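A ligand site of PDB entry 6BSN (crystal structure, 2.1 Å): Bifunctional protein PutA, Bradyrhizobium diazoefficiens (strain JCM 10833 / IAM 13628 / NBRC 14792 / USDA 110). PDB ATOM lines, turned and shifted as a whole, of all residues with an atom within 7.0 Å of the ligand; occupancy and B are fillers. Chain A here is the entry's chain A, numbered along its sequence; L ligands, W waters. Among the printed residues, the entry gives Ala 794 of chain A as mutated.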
ATOM      1  N   GLU A 613     -22.424 -12.662  30.099  1.00  0.00           N
ATOM      2  CA  GLU A 613     -22.645 -11.311  30.607  1.00  0.00           C
ATOM      3  C   GLU A 613     -23.857 -11.258  31.535  1.00  0.00           C
ATOM      4  O   GLU A 613     -23.832 -10.564  32.559  1.00  0.00           O
ATOM      5  CB  GLU A 613     -22.812 -10.353  29.419  1.00  0.00           C
ATOM      6  CG  GLU A 613     -22.843  -8.871  29.775  1.00  0.00           C
ATOM      7  CD  GLU A 613     -23.112  -7.981  28.559  1.00  0.00           C
ATOM      8  OE1 GLU A 613     -22.530  -8.261  27.496  1.00  0.00           O
ATOM      9  OE2 GLU A 613     -23.858  -6.994  28.676  1.00  0.00           O
ATOM     10  N   PHE A 617     -23.558 -10.056  35.312  1.00  0.00           N
ATOM     11  CA  PHE A 617     -24.372  -8.992  35.926  1.00  0.00           C
ATOM     12  C   PHE A 617     -24.972  -9.446  37.257  1.00  0.00           C
ATOM     13  O   PHE A 617     -24.896  -8.739  38.260  1.00  0.00           O
ATOM     14  CB  PHE A 617     -25.499  -8.559  34.980  1.00  0.00           C
ATOM     15  CG  PHE A 617     -25.144  -7.467  33.997  1.00  0.00           C
ATOM     16  CD1 PHE A 617     -25.424  -7.621  32.654  1.00  0.00           C
ATOM     17  CD2 PHE A 617     -24.602  -6.265  34.432  1.00  0.00           C
ATOM     18  CE1 PHE A 617     -25.099  -6.613  31.739  1.00  0.00           C
ATOM     19  CE2 PHE A 617     -24.289  -5.258  33.533  1.00  0.00           C
ATOM     20  CZ  PHE A 617     -24.524  -5.436  32.184  1.00  0.00           C
ATOM     21  N   ASN A 660     -31.353  -5.827  21.284  1.00  0.00           N
ATOM     22  CA  ASN A 660     -30.040  -6.246  20.819  1.00  0.00           C
ATOM     23  C   ASN A 660     -29.206  -6.938  21.896  1.00  0.00           C
ATOM     24  O   ASN A 660     -28.244  -7.638  21.551  1.00  0.00           O
ATOM     25  CB  ASN A 660     -29.264  -5.064  20.240  1.00  0.00           C
ATOM     26  CG  ASN A 660     -29.555  -3.760  20.957  1.00  0.00           C
ATOM     27  OD1 ASN A 660     -28.845  -3.394  21.887  1.00  0.00           O
ATOM     28  ND2 ASN A 660     -30.613  -3.046  20.503  1.00  0.00           N
ATOM     29  N   PHE A 661     -29.544  -6.751  23.171  1.00  0.00           N
ATOM     30  CA  PHE A 661     -29.056  -7.593  24.260  1.00  0.00           C
ATOM     31  C   PHE A 661     -30.273  -7.975  25.101  1.00  0.00           C
ATOM     32  O   PHE A 661     -30.490  -7.484  26.215  1.00  0.00           O
ATOM     33  CB  PHE A 661     -27.963  -6.914  25.074  1.00  0.00           C
ATOM     34  CG  PHE A 661     -26.635  -6.861  24.357  1.00  0.00           C
ATOM     35  CD1 PHE A 661     -26.286  -5.771  23.589  1.00  0.00           C
ATOM     36  CD2 PHE A 661     -25.764  -7.946  24.420  1.00  0.00           C
ATOM     37  CE1 PHE A 661     -25.063  -5.741  22.901  1.00  0.00           C
ATOM     38  CE2 PHE A 661     -24.549  -7.931  23.750  1.00  0.00           C
ATOM     39  CZ  PHE A 661     -24.196  -6.833  22.985  1.00  0.00           C
ATOM     40  N   ILE A 665     -28.825  -7.187  29.057  1.00  0.00           N
ATOM     41  CA  ILE A 665     -29.208  -5.844  29.460  1.00  0.00           C
ATOM     42  C   ILE A 665     -30.573  -5.881  30.110  1.00  0.00           C
ATOM     43  O   ILE A 665     -30.841  -5.122  31.062  1.00  0.00           O
ATOM     44  CB  ILE A 665     -29.171  -4.872  28.270  1.00  0.00           C
ATOM     45  CG1 ILE A 665     -27.725  -4.526  27.970  1.00  0.00           C
ATOM     46  CG2 ILE A 665     -29.955  -3.609  28.571  1.00  0.00           C
ATOM     47  CD1 ILE A 665     -27.599  -3.462  26.902  1.00  0.00           C
ATOM     48  N   THR A 734     -32.781   1.570  28.236  1.00  0.00           N
ATOM     49  CA  THR A 734     -31.733   1.417  27.242  1.00  0.00           C
ATOM     50  C   THR A 734     -32.383   1.369  25.871  1.00  0.00           C
ATOM     51  O   THR A 734     -33.207   0.481  25.609  1.00  0.00           O
ATOM     52  CB  THR A 734     -30.906   0.157  27.505  1.00  0.00           C
ATOM     53  OG1 THR A 734     -30.329   0.254  28.810  1.00  0.00           O
ATOM     54  CG2 THR A 734     -29.761   0.047  26.491  1.00  0.00           C
ATOM     55  N   GLU A 760     -29.229   4.791  28.774  1.00  0.00           N
ATOM     56  CA  GLU A 760     -28.093   4.596  27.871  1.00  0.00           C
ATOM     57  C   GLU A 760     -28.645   4.626  26.448  1.00  0.00           C
ATOM     58  O   GLU A 760     -29.555   3.858  26.120  1.00  0.00           O
ATOM     59  CB  GLU A 760     -27.364   3.278  28.164  1.00  0.00           C
ATOM     60  CG  GLU A 760     -26.076   3.042  27.302  1.00  0.00           C
ATOM     61  CD  GLU A 760     -26.346   2.145  26.105  1.00  0.00           C
ATOM     62  OE1 GLU A 760     -26.249   0.914  26.260  1.00  0.00           O
ATOM     63  OE2 GLU A 760     -26.687   2.683  25.019  1.00  0.00           O
ATOM     64  N   GLN A 792     -25.097  -4.240  15.391  1.00  0.00           N
ATOM     65  CA  GLN A 792     -26.250  -4.009  16.272  1.00  0.00           C
ATOM     66  C   GLN A 792     -25.801  -3.978  17.736  1.00  0.00           C
ATOM     67  O   GLN A 792     -26.232  -4.768  18.580  1.00  0.00           O
ATOM     68  CB  GLN A 792     -27.335  -5.065  16.023  1.00  0.00           C
ATOM     69  CG  GLN A 792     -27.914  -5.028  14.605  1.00  0.00           C
ATOM     70  CD  GLN A 792     -29.045  -6.043  14.376  1.00  0.00           C
ATOM     71  OE1 GLN A 792     -30.089  -5.725  13.806  1.00  0.00           O
ATOM     72  NE2 GLN A 792     -28.825  -7.259  14.827  1.00  0.00           N
ATOM     73  N   ARG A 793     -24.913  -3.028  18.018  1.00  0.00           N
ATOM     74  CA  ARG A 793     -24.381  -2.806  19.354  1.00  0.00           C
ATOM     75  C   ARG A 793     -24.236  -1.310  19.557  1.00  0.00           C
ATOM     76  O   ARG A 793     -23.806  -0.596  18.652  1.00  0.00           O
ATOM     77  CB  ARG A 793     -23.003  -3.448  19.559  1.00  0.00           C
ATOM     78  CG  ARG A 793     -22.951  -4.950  19.554  1.00  0.00           C
ATOM     79  CD  ARG A 793     -21.495  -5.374  19.681  1.00  0.00           C
ATOM     80  NE  ARG A 793     -21.313  -6.823  19.749  1.00  0.00           N
ATOM     81  CZ  ARG A 793     -21.007  -7.490  20.853  1.00  0.00           C
ATOM     82  NH1 ARG A 793     -20.844  -6.832  21.999  1.00  0.00           N
ATOM     83  NH2 ARG A 793     -20.869  -8.809  20.824  1.00  0.00           N
ATOM     84  N   ALA A 794     -24.592  -0.839  20.750  1.00  0.00           N
ATOM     85  CA  ALA A 794     -24.489   0.587  21.027  1.00  0.00           C
ATOM     86  C   ALA A 794     -23.037   1.044  21.018  1.00  0.00           C
ATOM     87  O   ALA A 794     -22.754   2.219  20.749  1.00  0.00           O
ATOM     88  CB  ALA A 794     -25.141   0.914  22.376  1.00  0.00           C
ATOM     89  N   SER A 795     -22.114   0.127  21.299  1.00  0.00           N
ATOM     90  CA  SER A 795     -20.679   0.370  21.364  1.00  0.00           C
ATOM     91  C   SER A 795     -19.985   0.334  20.009  1.00  0.00           C
ATOM     92  O   SER A 795     -18.779   0.589  19.943  1.00  0.00           O
ATOM     93  CB  SER A 795     -20.038  -0.690  22.252  1.00  0.00           C
ATOM     94  OG  SER A 795     -20.321  -1.988  21.704  1.00  0.00           O
ATOM     95  N   ALA A 796     -20.684  -0.040  18.945  1.00  0.00           N
ATOM     96  CA  ALA A 796     -20.035  -0.392  17.693  1.00  0.00           C
ATOM     97  C   ALA A 796     -19.329   0.806  17.072  1.00  0.00           C
ATOM     98  O   ALA A 796     -19.753   1.957  17.224  1.00  0.00           O
ATOM     99  CB  ALA A 796     -21.053  -0.936  16.699  1.00  0.00           C
ATOM    100  N   LEU A 916     -20.004   7.586  23.843  1.00  0.00           N
ATOM    101  CA  LEU A 916     -20.133   6.242  24.422  1.00  0.00           C
ATOM    102  C   LEU A 916     -18.804   5.496  24.328  1.00  0.00           C
ATOM    103  O   LEU A 916     -18.125   5.323  25.346  1.00  0.00           O
ATOM    104  CB  LEU A 916     -21.263   5.470  23.734  1.00  0.00           C
ATOM    105  CG  LEU A 916     -21.705   4.165  24.413  1.00  0.00           C
ATOM    106  CD1 LEU A 916     -21.887   4.350  25.943  1.00  0.00           C
ATOM    107  CD2 LEU A 916     -22.977   3.634  23.796  1.00  0.00           C
ATOM    108  N   THR A 917     -18.409   5.032  23.142  1.00  0.00           N
ATOM    109  CA  THR A 917     -17.086   4.419  22.996  1.00  0.00           C
ATOM    110  C   THR A 917     -16.199   5.218  22.044  1.00  0.00           C
ATOM    111  O   THR A 917     -16.674   5.994  21.204  1.00  0.00           O
ATOM    112  CB  THR A 917     -17.172   2.958  22.535  1.00  0.00           C
ATOM    113  OG1 THR A 917     -17.830   2.894  21.273  1.00  0.00           O
ATOM    114  CG2 THR A 917     -17.960   2.126  23.550  1.00  0.00           C
ATOM    115  N   TYR A 941     -11.046   2.647  24.447  1.00  0.00           N
ATOM    116  CA  TYR A 941     -10.373   1.377  24.197  1.00  0.00           C
ATOM    117  C   TYR A 941      -9.128   1.640  23.351  1.00  0.00           C
ATOM    118  O   TYR A 941      -9.246   2.173  22.237  1.00  0.00           O
ATOM    119  CB  TYR A 941     -11.294   0.407  23.473  1.00  0.00           C
ATOM    120  CG  TYR A 941     -12.433  -0.148  24.291  1.00  0.00           C
ATOM    121  CD1 TYR A 941     -13.713   0.357  24.160  1.00  0.00           C
ATOM    122  CD2 TYR A 941     -12.236  -1.224  25.153  1.00  0.00           C
ATOM    123  CE1 TYR A 941     -14.759  -0.167  24.877  1.00  0.00           C
ATOM    124  CE2 TYR A 941     -13.271  -1.748  25.892  1.00  0.00           C
ATOM    125  CZ  TYR A 941     -14.541  -1.219  25.747  1.00  0.00           C
ATOM    126  OH  TYR A 941     -15.603  -1.731  26.477  1.00  0.00           O
ATOM    127  N   MET A 946     -13.605  -2.198  20.333  1.00  0.00           N
ATOM    128  CA  MET A 946     -14.379  -1.277  21.168  1.00  0.00           C
ATOM    129  C   MET A 946     -15.619  -1.909  21.779  1.00  0.00           C
ATOM    130  O   MET A 946     -16.438  -1.203  22.369  1.00  0.00           O
ATOM    131  CB  MET A 946     -14.789  -0.059  20.320  1.00  0.00           C
ATOM    132  CG  MET A 946     -13.611   0.755  19.811  1.00  0.00           C
ATOM    133  SD  MET A 946     -14.003   1.743  18.354  1.00  0.00           S
ATOM    134  CE  MET A 946     -15.481   2.656  18.864  1.00  0.00           C
ATOM    135  N   ILE A 947     -15.776  -3.225  21.666  1.00  0.00           N
ATOM    136  CA  ILE A 947     -17.035  -3.886  21.961  1.00  0.00           C
ATOM    137  C   ILE A 947     -16.825  -4.971  23.039  1.00  0.00           C
ATOM    138  O   ILE A 947     -15.698  -5.314  23.402  1.00  0.00           O
ATOM    139  CB  ILE A 947     -17.655  -4.509  20.696  1.00  0.00           C
ATOM    140  CG1 ILE A 947     -16.730  -5.588  20.145  1.00  0.00           C
ATOM    141  CG2 ILE A 947     -17.956  -3.450  19.644  1.00  0.00           C
ATOM    142  CD1 ILE A 947     -17.411  -6.417  19.115  1.00  0.00           C
ATOM    143  N   GLY A 948     -17.926  -5.534  23.499  1.00  0.00           N
ATOM    144  CA  GLY A 948     -17.848  -6.609  24.486  1.00  0.00           C
ATOM    145  C   GLY A 948     -17.348  -6.191  25.859  1.00  0.00           C
ATOM    146  O   GLY A 948     -16.564  -6.920  26.465  1.00  0.00           O
ATOM    147  N   ALA A 949     -17.818  -5.047  26.387  1.00  0.00           N
ATOM    148  CA  ALA A 949     -17.452  -4.645  27.741  1.00  0.00           C
ATOM    149  C   ALA A 949     -17.754  -5.770  28.736  1.00  0.00           C
ATOM    150  O   ALA A 949     -18.774  -6.453  28.627  1.00  0.00           O
ATOM    151  CB  ALA A 949     -18.179  -3.366  28.129  1.00  0.00           C
ATOM    152  N   VAL A 950     -16.848  -5.984  29.674  1.00  0.00           N
ATOM    153  CA  VAL A 950     -16.973  -7.068  30.649  1.00  0.00           C
ATOM    154  C   VAL A 950     -17.439  -6.479  31.976  1.00  0.00           C
ATOM    155  O   VAL A 950     -16.830  -5.543  32.496  1.00  0.00           O
ATOM    156  CB  VAL A 950     -15.652  -7.841  30.805  1.00  0.00           C
ATOM    157  CG1 VAL A 950     -15.772  -8.846  31.950  1.00  0.00           C
ATOM    158  CG2 VAL A 950     -15.302  -8.590  29.469  1.00  0.00           C
ATOM    159  N   PHE A 956     -19.588   0.195  31.756  1.00  0.00           N
ATOM    160  CA  PHE A 956     -20.024   0.640  30.439  1.00  0.00           C
ATOM    161  C   PHE A 956     -21.059   1.761  30.534  1.00  0.00           C
ATOM    162  O   PHE A 956     -22.073   1.620  31.221  1.00  0.00           O
ATOM    163  CB  PHE A 956     -20.597  -0.529  29.622  1.00  0.00           C
ATOM    164  CG  PHE A 956     -20.978  -0.124  28.216  1.00  0.00           C
ATOM    165  CD1 PHE A 956     -22.291   0.255  27.914  1.00  0.00           C
ATOM    166  CD2 PHE A 956     -20.008  -0.080  27.210  1.00  0.00           C
ATOM    167  CE1 PHE A 956     -22.630   0.665  26.607  1.00  0.00           C
ATOM    168  CE2 PHE A 956     -20.340   0.325  25.908  1.00  0.00           C
ATOM    169  CZ  PHE A 956     -21.646   0.700  25.611  1.00  0.00           C
ATOM    170  N   ALA A 968     -23.245   0.995  33.760  1.00  0.00           N
ATOM    171  CA  ALA A 968     -23.647  -0.374  34.050  1.00  0.00           C
ATOM    172  C   ALA A 968     -22.425  -1.245  34.281  1.00  0.00           C
ATOM    173  O   ALA A 968     -21.384  -1.065  33.646  1.00  0.00           O
ATOM    174  CB  ALA A 968     -24.469  -0.924  32.877  1.00  0.00           C
HETATM  175  N1  LIG L   1     -22.460  -4.146  25.980  1.00  0.00           N
HETATM  176  C1  LIG L   1     -22.297  -3.917  24.552  1.00  0.00           C
HETATM  177  C2  LIG L   1     -20.802  -3.918  24.184  1.00  0.00           C
HETATM  178  O1  LIG L   1     -19.943  -3.581  25.037  1.00  0.00           O
HETATM  179  C3  LIG L   1     -22.936  -2.613  24.163  1.00  0.00           C
HETATM  180  C4  LIG L   1     -23.810  -2.273  25.373  1.00  0.00           C
HETATM  181  C5  LIG L   1     -23.123  -3.020  26.569  1.00  0.00           C
HETATM  182  O2  LIG L   1     -20.436  -4.229  23.032  1.00  0.00           O
HETATM  183  O   HOH W   1     -17.796  -1.707  24.864  1.00  0.00           O
HETATM  184  O   HOH W   2     -20.940  -6.150  26.529  1.00  0.00           O
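OG of Ser 795 lies within hydrogen-bond range of O2 of the ligand (2.6 Å).
NH1 of Arg 793 lies within salt-bridge range of O2 of the ligand (2.8 Å).
The backbone NH (N) of Gly 948 lies within hydrogen-bond range of an oxygen (O2) of the ligand.
An oxygen (O1) of the ligand lies within hydrogen-bond range of the backbone NH (N) of Ala 949 (2.9 Å).
OG1 of Thr 917 sits at hydrogen-bond distance from O of Ser 795 (2.8 Å).
O of Phe 956 lies within hydrogen-bond range of N of Ala 968 (2.9 Å).
Residues that only touch the ligand: Phe 661, Ile 947 and Phe 956.
Hydrophobic or aromatic side chains within 4 Å of the ligand: Phe 661, Ile 947, Ala 949 and Phe 956.
Within 4 Å of the ligand: Phe 661, Arg 793, Ser 795, Ile 947, Gly 948, Ala 949 and Phe 956.
Water W2 lies within hydrogen-bond range of N1 of the ligand (2.6 Å), OE1 of Glu 613 (2.8 Å) and O of Ala 949 (3.0 Å).
Water W1 lies within hydrogen-bond range of the side-chain hydroxyl of Tyr 941 (2.7 Å), an oxygen (O1) of the ligand (2.9 Å) and the backbone carbonyl oxygen of Met 946 (2.9 Å).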
